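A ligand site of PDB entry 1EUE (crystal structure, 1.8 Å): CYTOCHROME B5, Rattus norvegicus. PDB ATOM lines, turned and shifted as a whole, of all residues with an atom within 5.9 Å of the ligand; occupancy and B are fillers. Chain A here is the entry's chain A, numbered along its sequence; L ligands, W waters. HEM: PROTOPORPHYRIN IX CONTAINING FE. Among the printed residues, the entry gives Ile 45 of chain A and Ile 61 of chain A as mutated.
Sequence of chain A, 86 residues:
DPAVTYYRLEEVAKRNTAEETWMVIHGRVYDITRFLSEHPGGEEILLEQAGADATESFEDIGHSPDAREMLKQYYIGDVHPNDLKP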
ATOM      1  N   MET A  23      -5.758   8.948  -9.978  1.00  0.00           N
ATOM      2  CA  MET A  23      -4.774   8.487 -10.928  1.00  0.00           C
ATOM      3  C   MET A  23      -3.417   8.549 -10.235  1.00  0.00           C
ATOM      4  O   MET A  23      -3.198   9.408  -9.385  1.00  0.00           O
ATOM      5  CB  MET A  23      -4.784   9.432 -12.121  1.00  0.00           C
ATOM      6  CG  MET A  23      -3.899   9.066 -13.253  1.00  0.00           C
ATOM      7  SD  MET A  23      -4.201  10.251 -14.586  1.00  0.00           S
ATOM      8  CE  MET A  23      -5.559   9.494 -15.378  1.00  0.00           C
ATOM      9  N   ILE A  25       0.689   8.941 -10.655  1.00  0.00           N
ATOM     10  CA  ILE A  25       1.726   9.463 -11.546  1.00  0.00           C
ATOM     11  C   ILE A  25       2.993   9.547 -10.696  1.00  0.00           C
ATOM     12  O   ILE A  25       3.011  10.240  -9.676  1.00  0.00           O
ATOM     13  CB  ILE A  25       1.384  10.859 -12.099  1.00  0.00           C
ATOM     14  CG1 ILE A  25       0.115  10.771 -12.962  1.00  0.00           C
ATOM     15  CG2 ILE A  25       2.554  11.395 -12.918  1.00  0.00           C
ATOM     16  CD1 ILE A  25      -0.352  12.103 -13.484  1.00  0.00           C
ATOM     17  N   TYR A  30      -3.366  11.299  -7.279  1.00  0.00           N
ATOM     18  CA  TYR A  30      -4.008  12.577  -7.586  1.00  0.00           C
ATOM     19  C   TYR A  30      -5.499  12.366  -7.783  1.00  0.00           C
ATOM     20  O   TYR A  30      -5.913  11.439  -8.485  1.00  0.00           O
ATOM     21  CB  TYR A  30      -3.417  13.183  -8.868  1.00  0.00           C
ATOM     22  CG  TYR A  30      -1.959  13.483  -8.751  1.00  0.00           C
ATOM     23  CD1 TYR A  30      -0.999  12.509  -9.074  1.00  0.00           C
ATOM     24  CD2 TYR A  30      -1.515  14.700  -8.226  1.00  0.00           C
ATOM     25  CE1 TYR A  30       0.378  12.761  -8.863  1.00  0.00           C
ATOM     26  CE2 TYR A  30      -0.160  14.953  -8.020  1.00  0.00           C
ATOM     27  CZ  TYR A  30       0.787  13.976  -8.347  1.00  0.00           C
ATOM     28  OH  TYR A  30       2.133  14.234  -8.162  1.00  0.00           O
ATOM     29  N   ILE A  32      -8.284  13.735  -9.616  1.00  0.00           N
ATOM     30  CA  ILE A  32      -8.498  14.659 -10.731  1.00  0.00           C
ATOM     31  C   ILE A  32      -9.973  14.816 -11.118  1.00  0.00           C
ATOM     32  O   ILE A  32     -10.272  15.308 -12.201  1.00  0.00           O
ATOM     33  CB  ILE A  32      -7.678  14.216 -11.981  1.00  0.00           C
ATOM     34  CG1 ILE A  32      -8.009  12.765 -12.338  1.00  0.00           C
ATOM     35  CG2 ILE A  32      -6.138  14.370 -11.686  1.00  0.00           C
ATOM     36  CD1 ILE A  32      -7.648  12.358 -13.746  1.00  0.00           C
ATOM     37  N   PHE A  35     -10.896  18.070 -12.422  1.00  0.00           N
ATOM     38  CA  PHE A  35     -10.060  18.518 -13.527  1.00  0.00           C
ATOM     39  C   PHE A  35     -10.506  17.921 -14.862  1.00  0.00           C
ATOM     40  O   PHE A  35     -10.116  18.406 -15.920  1.00  0.00           O
ATOM     41  CB  PHE A  35      -8.598  18.129 -13.236  1.00  0.00           C
ATOM     42  CG  PHE A  35      -7.644  18.458 -14.355  1.00  0.00           C
ATOM     43  CD1 PHE A  35      -7.355  19.777 -14.683  1.00  0.00           C
ATOM     44  CD2 PHE A  35      -6.999  17.431 -15.044  1.00  0.00           C
ATOM     45  CE1 PHE A  35      -6.427  20.078 -15.687  1.00  0.00           C
ATOM     46  CE2 PHE A  35      -6.073  17.728 -16.038  1.00  0.00           C
ATOM     47  CZ  PHE A  35      -5.781  19.051 -16.353  1.00  0.00           C
ATOM     48  N   HIS A  39      -9.208  19.513 -18.640  1.00  0.00           N
ATOM     49  CA  HIS A  39      -8.041  18.968 -19.306  1.00  0.00           C
ATOM     50  C   HIS A  39      -7.990  19.293 -20.806  1.00  0.00           C
ATOM     51  O   HIS A  39      -8.898  18.927 -21.552  1.00  0.00           O
ATOM     52  CB  HIS A  39      -8.025  17.459 -19.114  1.00  0.00           C
ATOM     53  CG  HIS A  39      -6.819  16.795 -19.700  1.00  0.00           C
ATOM     54  ND1 HIS A  39      -6.916  15.657 -20.467  1.00  0.00           N
ATOM     55  CD2 HIS A  39      -5.505  17.081 -19.600  1.00  0.00           C
ATOM     56  CE1 HIS A  39      -5.694  15.273 -20.823  1.00  0.00           C
ATOM     57  NE2 HIS A  39      -4.828  16.134 -20.302  1.00  0.00           N
ATOM     58  N   PRO A  40      -6.931  19.978 -21.271  1.00  0.00           N
ATOM     59  CA  PRO A  40      -6.866  20.285 -22.710  1.00  0.00           C
ATOM     60  C   PRO A  40      -6.867  19.054 -23.607  1.00  0.00           C
ATOM     61  O   PRO A  40      -7.289  19.129 -24.759  1.00  0.00           O
ATOM     62  CB  PRO A  40      -5.580  21.090 -22.843  1.00  0.00           C
ATOM     63  CG  PRO A  40      -5.507  21.818 -21.538  1.00  0.00           C
ATOM     64  CD  PRO A  40      -5.937  20.755 -20.523  1.00  0.00           C
ATOM     65  N   GLY A  41      -6.377  17.913 -23.107  1.00  0.00           N
ATOM     66  CA  GLY A  41      -6.382  16.715 -23.924  1.00  0.00           C
ATOM     67  C   GLY A  41      -7.726  15.972 -23.910  1.00  0.00           C
ATOM     68  O   GLY A  41      -7.870  14.914 -24.529  1.00  0.00           O
ATOM     69  N   ILE A  45      -9.664  10.552 -22.475  1.00  0.00           N
ATOM     70  CA  ILE A  45      -8.343   9.945 -22.381  1.00  0.00           C
ATOM     71  C   ILE A  45      -7.918   9.765 -20.917  1.00  0.00           C
ATOM     72  O   ILE A  45      -7.153   8.842 -20.590  1.00  0.00           O
ATOM     73  CB  ILE A  45      -7.324  10.771 -23.229  1.00  0.00           C
ATOM     74  CG1 ILE A  45      -6.146   9.863 -23.629  1.00  0.00           C
ATOM     75  CG2 ILE A  45      -6.853  12.012 -22.463  1.00  0.00           C
ATOM     76  CD1 ILE A  45      -5.284  10.444 -24.746  1.00  0.00           C
ATOM     77  N   LEU A  46      -8.436  10.605 -20.024  1.00  0.00           N
ATOM     78  CA  LEU A  46      -8.134  10.471 -18.591  1.00  0.00           C
ATOM     79  C   LEU A  46      -8.966   9.342 -17.969  1.00  0.00           C
ATOM     80  O   LEU A  46      -8.484   8.540 -17.162  1.00  0.00           O
ATOM     81  CB  LEU A  46      -8.423  11.799 -17.852  1.00  0.00           C
ATOM     82  CG  LEU A  46      -7.614  13.030 -18.276  1.00  0.00           C
ATOM     83  CD1 LEU A  46      -8.066  14.267 -17.493  1.00  0.00           C
ATOM     84  CD2 LEU A  46      -6.149  12.772 -18.015  1.00  0.00           C
ATOM     85  N   GLN A  49      -7.708   5.803 -18.237  1.00  0.00           N
ATOM     86  CA  GLN A  49      -6.644   5.362 -17.345  1.00  0.00           C
ATOM     87  C   GLN A  49      -6.962   5.659 -15.875  1.00  0.00           C
ATOM     88  O   GLN A  49      -6.072   5.612 -15.038  1.00  0.00           O
ATOM     89  CB  GLN A  49      -5.330   6.011 -17.722  1.00  0.00           C
ATOM     90  CG  GLN A  49      -5.100   6.016 -19.212  1.00  0.00           C
ATOM     91  CD  GLN A  49      -3.656   5.832 -19.594  1.00  0.00           C
ATOM     92  OE1 GLN A  49      -3.269   6.228 -20.693  1.00  0.00           O
ATOM     93  NE2 GLN A  49      -2.867   5.220 -18.720  1.00  0.00           N
ATOM     94  N   ALA A  54      -0.736   6.037 -14.439  1.00  0.00           N
ATOM     95  CA  ALA A  54      -0.681   6.598 -15.777  1.00  0.00           C
ATOM     96  C   ALA A  54       0.630   7.305 -16.095  1.00  0.00           C
ATOM     97  O   ALA A  54       0.704   8.087 -17.016  1.00  0.00           O
ATOM     98  CB  ALA A  54      -1.846   7.579 -15.981  1.00  0.00           C
ATOM     99  N   SER A  57       1.948   7.082 -19.885  1.00  0.00           N
ATOM    100  CA  SER A  57       1.167   7.899 -20.811  1.00  0.00           C
ATOM    101  C   SER A  57       1.373   9.393 -20.588  1.00  0.00           C
ATOM    102  O   SER A  57       1.462  10.183 -21.536  1.00  0.00           O
ATOM    103  CB  SER A  57      -0.314   7.575 -20.687  1.00  0.00           C
ATOM    104  OG  SER A  57      -0.559   6.220 -20.981  1.00  0.00           O
ATOM    105  N   PHE A  58       1.432   9.803 -19.315  1.00  0.00           N
ATOM    106  CA  PHE A  58       1.620  11.220 -19.007  1.00  0.00           C
ATOM    107  C   PHE A  58       2.946  11.726 -19.590  1.00  0.00           C
ATOM    108  O   PHE A  58       3.004  12.830 -20.125  1.00  0.00           O
ATOM    109  CB  PHE A  58       1.607  11.428 -17.494  1.00  0.00           C
ATOM    110  CG  PHE A  58       1.839  12.862 -17.079  1.00  0.00           C
ATOM    111  CD1 PHE A  58       0.787  13.775 -17.029  1.00  0.00           C
ATOM    112  CD2 PHE A  58       3.106  13.289 -16.714  1.00  0.00           C
ATOM    113  CE1 PHE A  58       0.983  15.080 -16.623  1.00  0.00           C
ATOM    114  CE2 PHE A  58       3.326  14.617 -16.304  1.00  0.00           C
ATOM    115  CZ  PHE A  58       2.259  15.523 -16.249  1.00  0.00           C
ATOM    116  N   ILE A  61       3.283  11.689 -23.684  1.00  0.00           N
ATOM    117  CA  ILE A  61       2.631  12.827 -24.314  1.00  0.00           C
ATOM    118  C   ILE A  61       3.558  14.019 -24.426  1.00  0.00           C
ATOM    119  O   ILE A  61       3.508  14.782 -25.396  1.00  0.00           O
ATOM    120  CB  ILE A  61       1.358  13.236 -23.510  1.00  0.00           C
ATOM    121  CG1 ILE A  61       0.255  12.206 -23.736  1.00  0.00           C
ATOM    122  CG2 ILE A  61       0.936  14.649 -23.884  1.00  0.00           C
ATOM    123  CD1 ILE A  61      -0.081  11.962 -25.212  1.00  0.00           C
ATOM    124  N   HIS A  63       4.114  16.380 -21.671  1.00  0.00           N
ATOM    125  CA  HIS A  63       3.445  17.490 -20.995  1.00  0.00           C
ATOM    126  C   HIS A  63       4.443  18.597 -20.670  1.00  0.00           C
ATOM    127  O   HIS A  63       5.609  18.332 -20.359  1.00  0.00           O
ATOM    128  CB  HIS A  63       2.752  17.010 -19.703  1.00  0.00           C
ATOM    129  CG  HIS A  63       1.483  16.263 -19.954  1.00  0.00           C
ATOM    130  ND1 HIS A  63       1.454  14.908 -20.208  1.00  0.00           N
ATOM    131  CD2 HIS A  63       0.200  16.687 -20.031  1.00  0.00           C
ATOM    132  CE1 HIS A  63       0.206  14.535 -20.443  1.00  0.00           C
ATOM    133  NE2 HIS A  63      -0.573  15.596 -20.330  1.00  0.00           N
ATOM    134  N   SER A  64       3.964  19.837 -20.732  1.00  0.00           N
ATOM    135  CA  SER A  64       4.786  20.998 -20.446  1.00  0.00           C
ATOM    136  C   SER A  64       5.072  21.192 -18.947  1.00  0.00           C
ATOM    137  O   SER A  64       4.465  20.540 -18.082  1.00  0.00           O
ATOM    138  CB  SER A  64       4.080  22.245 -20.949  1.00  0.00           C
ATOM    139  OG  SER A  64       3.008  22.541 -20.071  1.00  0.00           O
ATOM    140  N   ASP A  66       4.287  23.652 -17.247  1.00  0.00           N
ATOM    141  CA  ASP A  66       3.085  24.217 -16.626  1.00  0.00           C
ATOM    142  C   ASP A  66       2.088  23.122 -16.285  1.00  0.00           C
ATOM    143  O   ASP A  66       1.394  23.213 -15.298  1.00  0.00           O
ATOM    144  CB  ASP A  66       2.427  25.242 -17.565  1.00  0.00           C
ATOM    145  CG  ASP A  66       3.303  26.467 -17.775  1.00  0.00           C
ATOM    146  OD1 ASP A  66       3.855  27.014 -16.786  1.00  0.00           O
ATOM    147  OD2 ASP A  66       3.432  26.891 -18.945  1.00  0.00           O
ATOM    148  N   ALA A  67       2.010  22.085 -17.114  1.00  0.00           N
ATOM    149  CA  ALA A  67       1.131  20.958 -16.850  1.00  0.00           C
ATOM    150  C   ALA A  67       1.591  20.256 -15.555  1.00  0.00           C
ATOM    151  O   ALA A  67       0.789  19.853 -14.713  1.00  0.00           O
ATOM    152  CB  ALA A  67       1.169  19.992 -18.024  1.00  0.00           C
ATOM    153  N   ARG A  68       2.902  20.072 -15.409  1.00  0.00           N
ATOM    154  CA  ARG A  68       3.422  19.440 -14.203  1.00  0.00           C
ATOM    155  C   ARG A  68       3.081  20.223 -12.958  1.00  0.00           C
ATOM    156  O   ARG A  68       2.794  19.657 -11.900  1.00  0.00           O
ATOM    157  CB  ARG A  68       4.949  19.302 -14.254  1.00  0.00           C
ATOM    158  CG  ARG A  68       5.423  18.446 -15.366  1.00  0.00           C
ATOM    159  CD  ARG A  68       6.899  18.126 -15.186  1.00  0.00           C
ATOM    160  NE  ARG A  68       7.406  17.461 -16.373  1.00  0.00           N
ATOM    161  CZ  ARG A  68       7.410  16.144 -16.547  1.00  0.00           C
ATOM    162  NH1 ARG A  68       6.938  15.342 -15.593  1.00  0.00           N
ATOM    163  NH2 ARG A  68       7.902  15.639 -17.665  1.00  0.00           N
ATOM    164  N   MET A  70       0.505  22.034 -12.449  1.00  0.00           N
ATOM    165  CA  MET A  70      -0.932  21.873 -12.163  1.00  0.00           C
ATOM    166  C   MET A  70      -1.186  20.675 -11.279  1.00  0.00           C
ATOM    167  O   MET A  70      -2.187  20.643 -10.565  1.00  0.00           O
ATOM    168  CB  MET A  70      -1.706  21.677 -13.462  1.00  0.00           C
ATOM    169  CG  MET A  70      -1.780  22.900 -14.322  1.00  0.00           C
ATOM    170  SD  MET A  70      -2.873  22.515 -15.702  1.00  0.00           S
ATOM    171  CE  MET A  70      -4.477  22.564 -14.869  1.00  0.00           C
ATOM    172  N   LEU A  71      -0.305  19.676 -11.329  1.00  0.00           N
ATOM    173  CA  LEU A  71      -0.479  18.480 -10.505  1.00  0.00           C
ATOM    174  C   LEU A  71      -0.606  18.730  -9.022  1.00  0.00           C
ATOM    175  O   LEU A  71      -1.359  18.041  -8.331  1.00  0.00           O
ATOM    176  CB  LEU A  71       0.700  17.530 -10.721  1.00  0.00           C
ATOM    177  CG  LEU A  71       0.662  16.656 -11.961  1.00  0.00           C
ATOM    178  CD1 LEU A  71       1.985  15.887 -12.073  1.00  0.00           C
ATOM    179  CD2 LEU A  71      -0.541  15.709 -11.859  1.00  0.00           C
ATOM    180  N   TYR A  74      -3.894  18.719  -7.154  1.00  0.00           N
ATOM    181  CA  TYR A  74      -4.672  17.486  -7.002  1.00  0.00           C
ATOM    182  C   TYR A  74      -4.028  16.373  -6.185  1.00  0.00           C
ATOM    183  O   TYR A  74      -4.614  15.306  -6.015  1.00  0.00           O
ATOM    184  CB  TYR A  74      -5.030  16.969  -8.404  1.00  0.00           C
ATOM    185  CG  TYR A  74      -5.645  18.052  -9.285  1.00  0.00           C
ATOM    186  CD1 TYR A  74      -6.915  18.559  -9.008  1.00  0.00           C
ATOM    187  CD2 TYR A  74      -4.936  18.599 -10.353  1.00  0.00           C
ATOM    188  CE1 TYR A  74      -7.467  19.587  -9.765  1.00  0.00           C
ATOM    189  CE2 TYR A  74      -5.492  19.644 -11.136  1.00  0.00           C
ATOM    190  CZ  TYR A  74      -6.752  20.126 -10.824  1.00  0.00           C
ATOM    191  OH  TYR A  74      -7.316  21.134 -11.558  1.00  0.00           O
HETATM  192  CHA HEM L   1      -2.568  18.250 -22.927  1.00  0.00           C
HETATM  193  CHB HEM L   1      -2.444  18.584 -18.099  1.00  0.00           C
HETATM  194  CHC HEM L   1      -2.791  13.788 -17.682  1.00  0.00           C
HETATM  195  CHD HEM L   1      -3.026  13.438 -22.509  1.00  0.00           C
HETATM  196  C1A HEM L   1      -2.466  18.758 -21.645  1.00  0.00           C
HETATM  197  C2A HEM L   1      -2.226  20.126 -21.346  1.00  0.00           C
HETATM  198  C3A HEM L   1      -2.205  20.231 -19.973  1.00  0.00           C
HETATM  199  C4A HEM L   1      -2.421  18.918 -19.435  1.00  0.00           C
HETATM  200  CMA HEM L   1      -2.010  21.424 -19.237  1.00  0.00           C
HETATM  201  CAA HEM L   1      -2.004  21.267 -22.364  1.00  0.00           C
HETATM  202  CBA HEM L   1      -0.514  21.232 -22.848  1.00  0.00           C
HETATM  203  CGA HEM L   1      -0.097  22.271 -23.854  1.00  0.00           C
HETATM  204  O1A HEM L   1       0.641  21.883 -24.830  1.00  0.00           O
HETATM  205  O2A HEM L   1      -0.468  23.477 -23.670  1.00  0.00           O
HETATM  206  C1B HEM L   1      -2.557  17.316 -17.606  1.00  0.00           C
HETATM  207  C2B HEM L   1      -2.564  17.009 -16.199  1.00  0.00           C
HETATM  208  C3B HEM L   1      -2.662  15.689 -16.029  1.00  0.00           C
HETATM  209  C4B HEM L   1      -2.714  15.148 -17.391  1.00  0.00           C
HETATM  210  CMB HEM L   1      -2.467  18.059 -15.102  1.00  0.00           C
HETATM  211  CAB HEM L   1      -2.682  14.982 -14.736  1.00  0.00           C
HETATM  212  CBB HEM L   1      -3.935  14.173 -14.450  1.00  0.00           C
HETATM  213  C1C HEM L   1      -2.834  13.263 -18.946  1.00  0.00           C
HETATM  214  C2C HEM L   1      -2.908  11.846 -19.250  1.00  0.00           C
HETATM  215  C3C HEM L   1      -3.009  11.718 -20.597  1.00  0.00           C
HETATM  216  C4C HEM L   1      -2.975  13.095 -21.138  1.00  0.00           C
HETATM  217  CMC HEM L   1      -2.898  10.672 -18.260  1.00  0.00           C
HETATM  218  CAC HEM L   1      -3.130  10.430 -21.391  1.00  0.00           C
HETATM  219  CBC HEM L   1      -2.248   9.973 -22.297  1.00  0.00           C
HETATM  220  C1D HEM L   1      -2.947  14.729 -23.033  1.00  0.00           C
HETATM  221  C2D HEM L   1      -3.000  15.029 -24.457  1.00  0.00           C
HETATM  222  C3D HEM L   1      -2.859  16.386 -24.601  1.00  0.00           C
HETATM  223  C4D HEM L   1      -2.742  16.901 -23.234  1.00  0.00           C
HETATM  224  CMD HEM L   1      -3.179  14.017 -25.590  1.00  0.00           C
HETATM  225  CAD HEM L   1      -2.839  17.199 -25.924  1.00  0.00           C
HETATM  226  CBD HEM L   1      -1.390  17.552 -26.357  1.00  0.00           C
HETATM  227  CGD HEM L   1      -1.318  18.104 -27.762  1.00  0.00           C
HETATM  228  O1D HEM L   1      -1.857  19.214 -27.986  1.00  0.00           O
HETATM  229  O2D HEM L   1      -0.739  17.399 -28.637  1.00  0.00           O
HETATM  230  NA  HEM L   1      -2.553  17.992 -20.473  1.00  0.00           N
HETATM  231  NB  HEM L   1      -2.660  16.165 -18.369  1.00  0.00           N
HETATM  232  NC  HEM L   1      -2.849  14.049 -20.099  1.00  0.00           N
HETATM  233  ND  HEM L   1      -2.808  15.881 -22.261  1.00  0.00           N
HETATM  234 FE   HEM L   1      -2.718  16.022 -20.306  1.00  0.00          FE
HETATM  235  O   HOH W   1      -0.100  24.483 -21.264  1.00  0.00           O
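An iron atom (FE) of the ligand is bound by a ring nitrogen (NE2) of His 63 (2.2 Å).
A ring nitrogen (NE2) of His 39 is bound to an iron atom (FE) of the ligand.
The side-chain amide oxygen (OE1) of Gln 49 lies within hydrogen-bond range of the side-chain hydroxyl (OG) of Ser 57 (2.7 Å).
The backbone carbonyl oxygen (O) of Phe 58 sits at hydrogen-bond distance from a ring nitrogen (ND1) of His 63.
The backbone carbonyl oxygen of Met 23 lies within hydrogen-bond range of the backbone NH of Tyr 30 (2.8 Å).
N of Ala 67 lies within hydrogen-bond range of OG of Ser 64 (3.2 Å).
Met 23 touches the ligand.
Ile 25 touches the ligand.
Ile 32 touches the ligand (CG2 to CBB, 3.5 Å).
Phe 35 touches the ligand.
CB of Pro 40 touches CAA of the ligand, 3.6 Å away.
CA of Gly 41 touches C3D of the ligand, 3.6 Å away.
CG1 of Ile 45 touches CAC of the ligand, at 3.8 Å.
Leu 46 touches the ligand (CD2 to C1C, 3.5 Å).
Ala 54 touches the ligand (CB to CMC, 3.98 Å).
CB of Ser 57 touches CBC of the ligand, 3.5 Å away.
Phe 58 touches the ligand.
Ile 61 touches the ligand (CG1 to CBC, 3.6 Å).
Ala 67 touches the ligand (CB to CMA, 3.7 Å).
Met 70 touches the ligand.
CD2 of Leu 71 touches CAB of the ligand, 3.7 Å away.
Of the 23 residues printed, 17 come within 4 Å of the ligand.
Along chain A the residues within 4 Å of the ligand span positions 23 to 71.
The nearest printed residue that does not touch the ligand is Gln 49 (4.2 Å).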
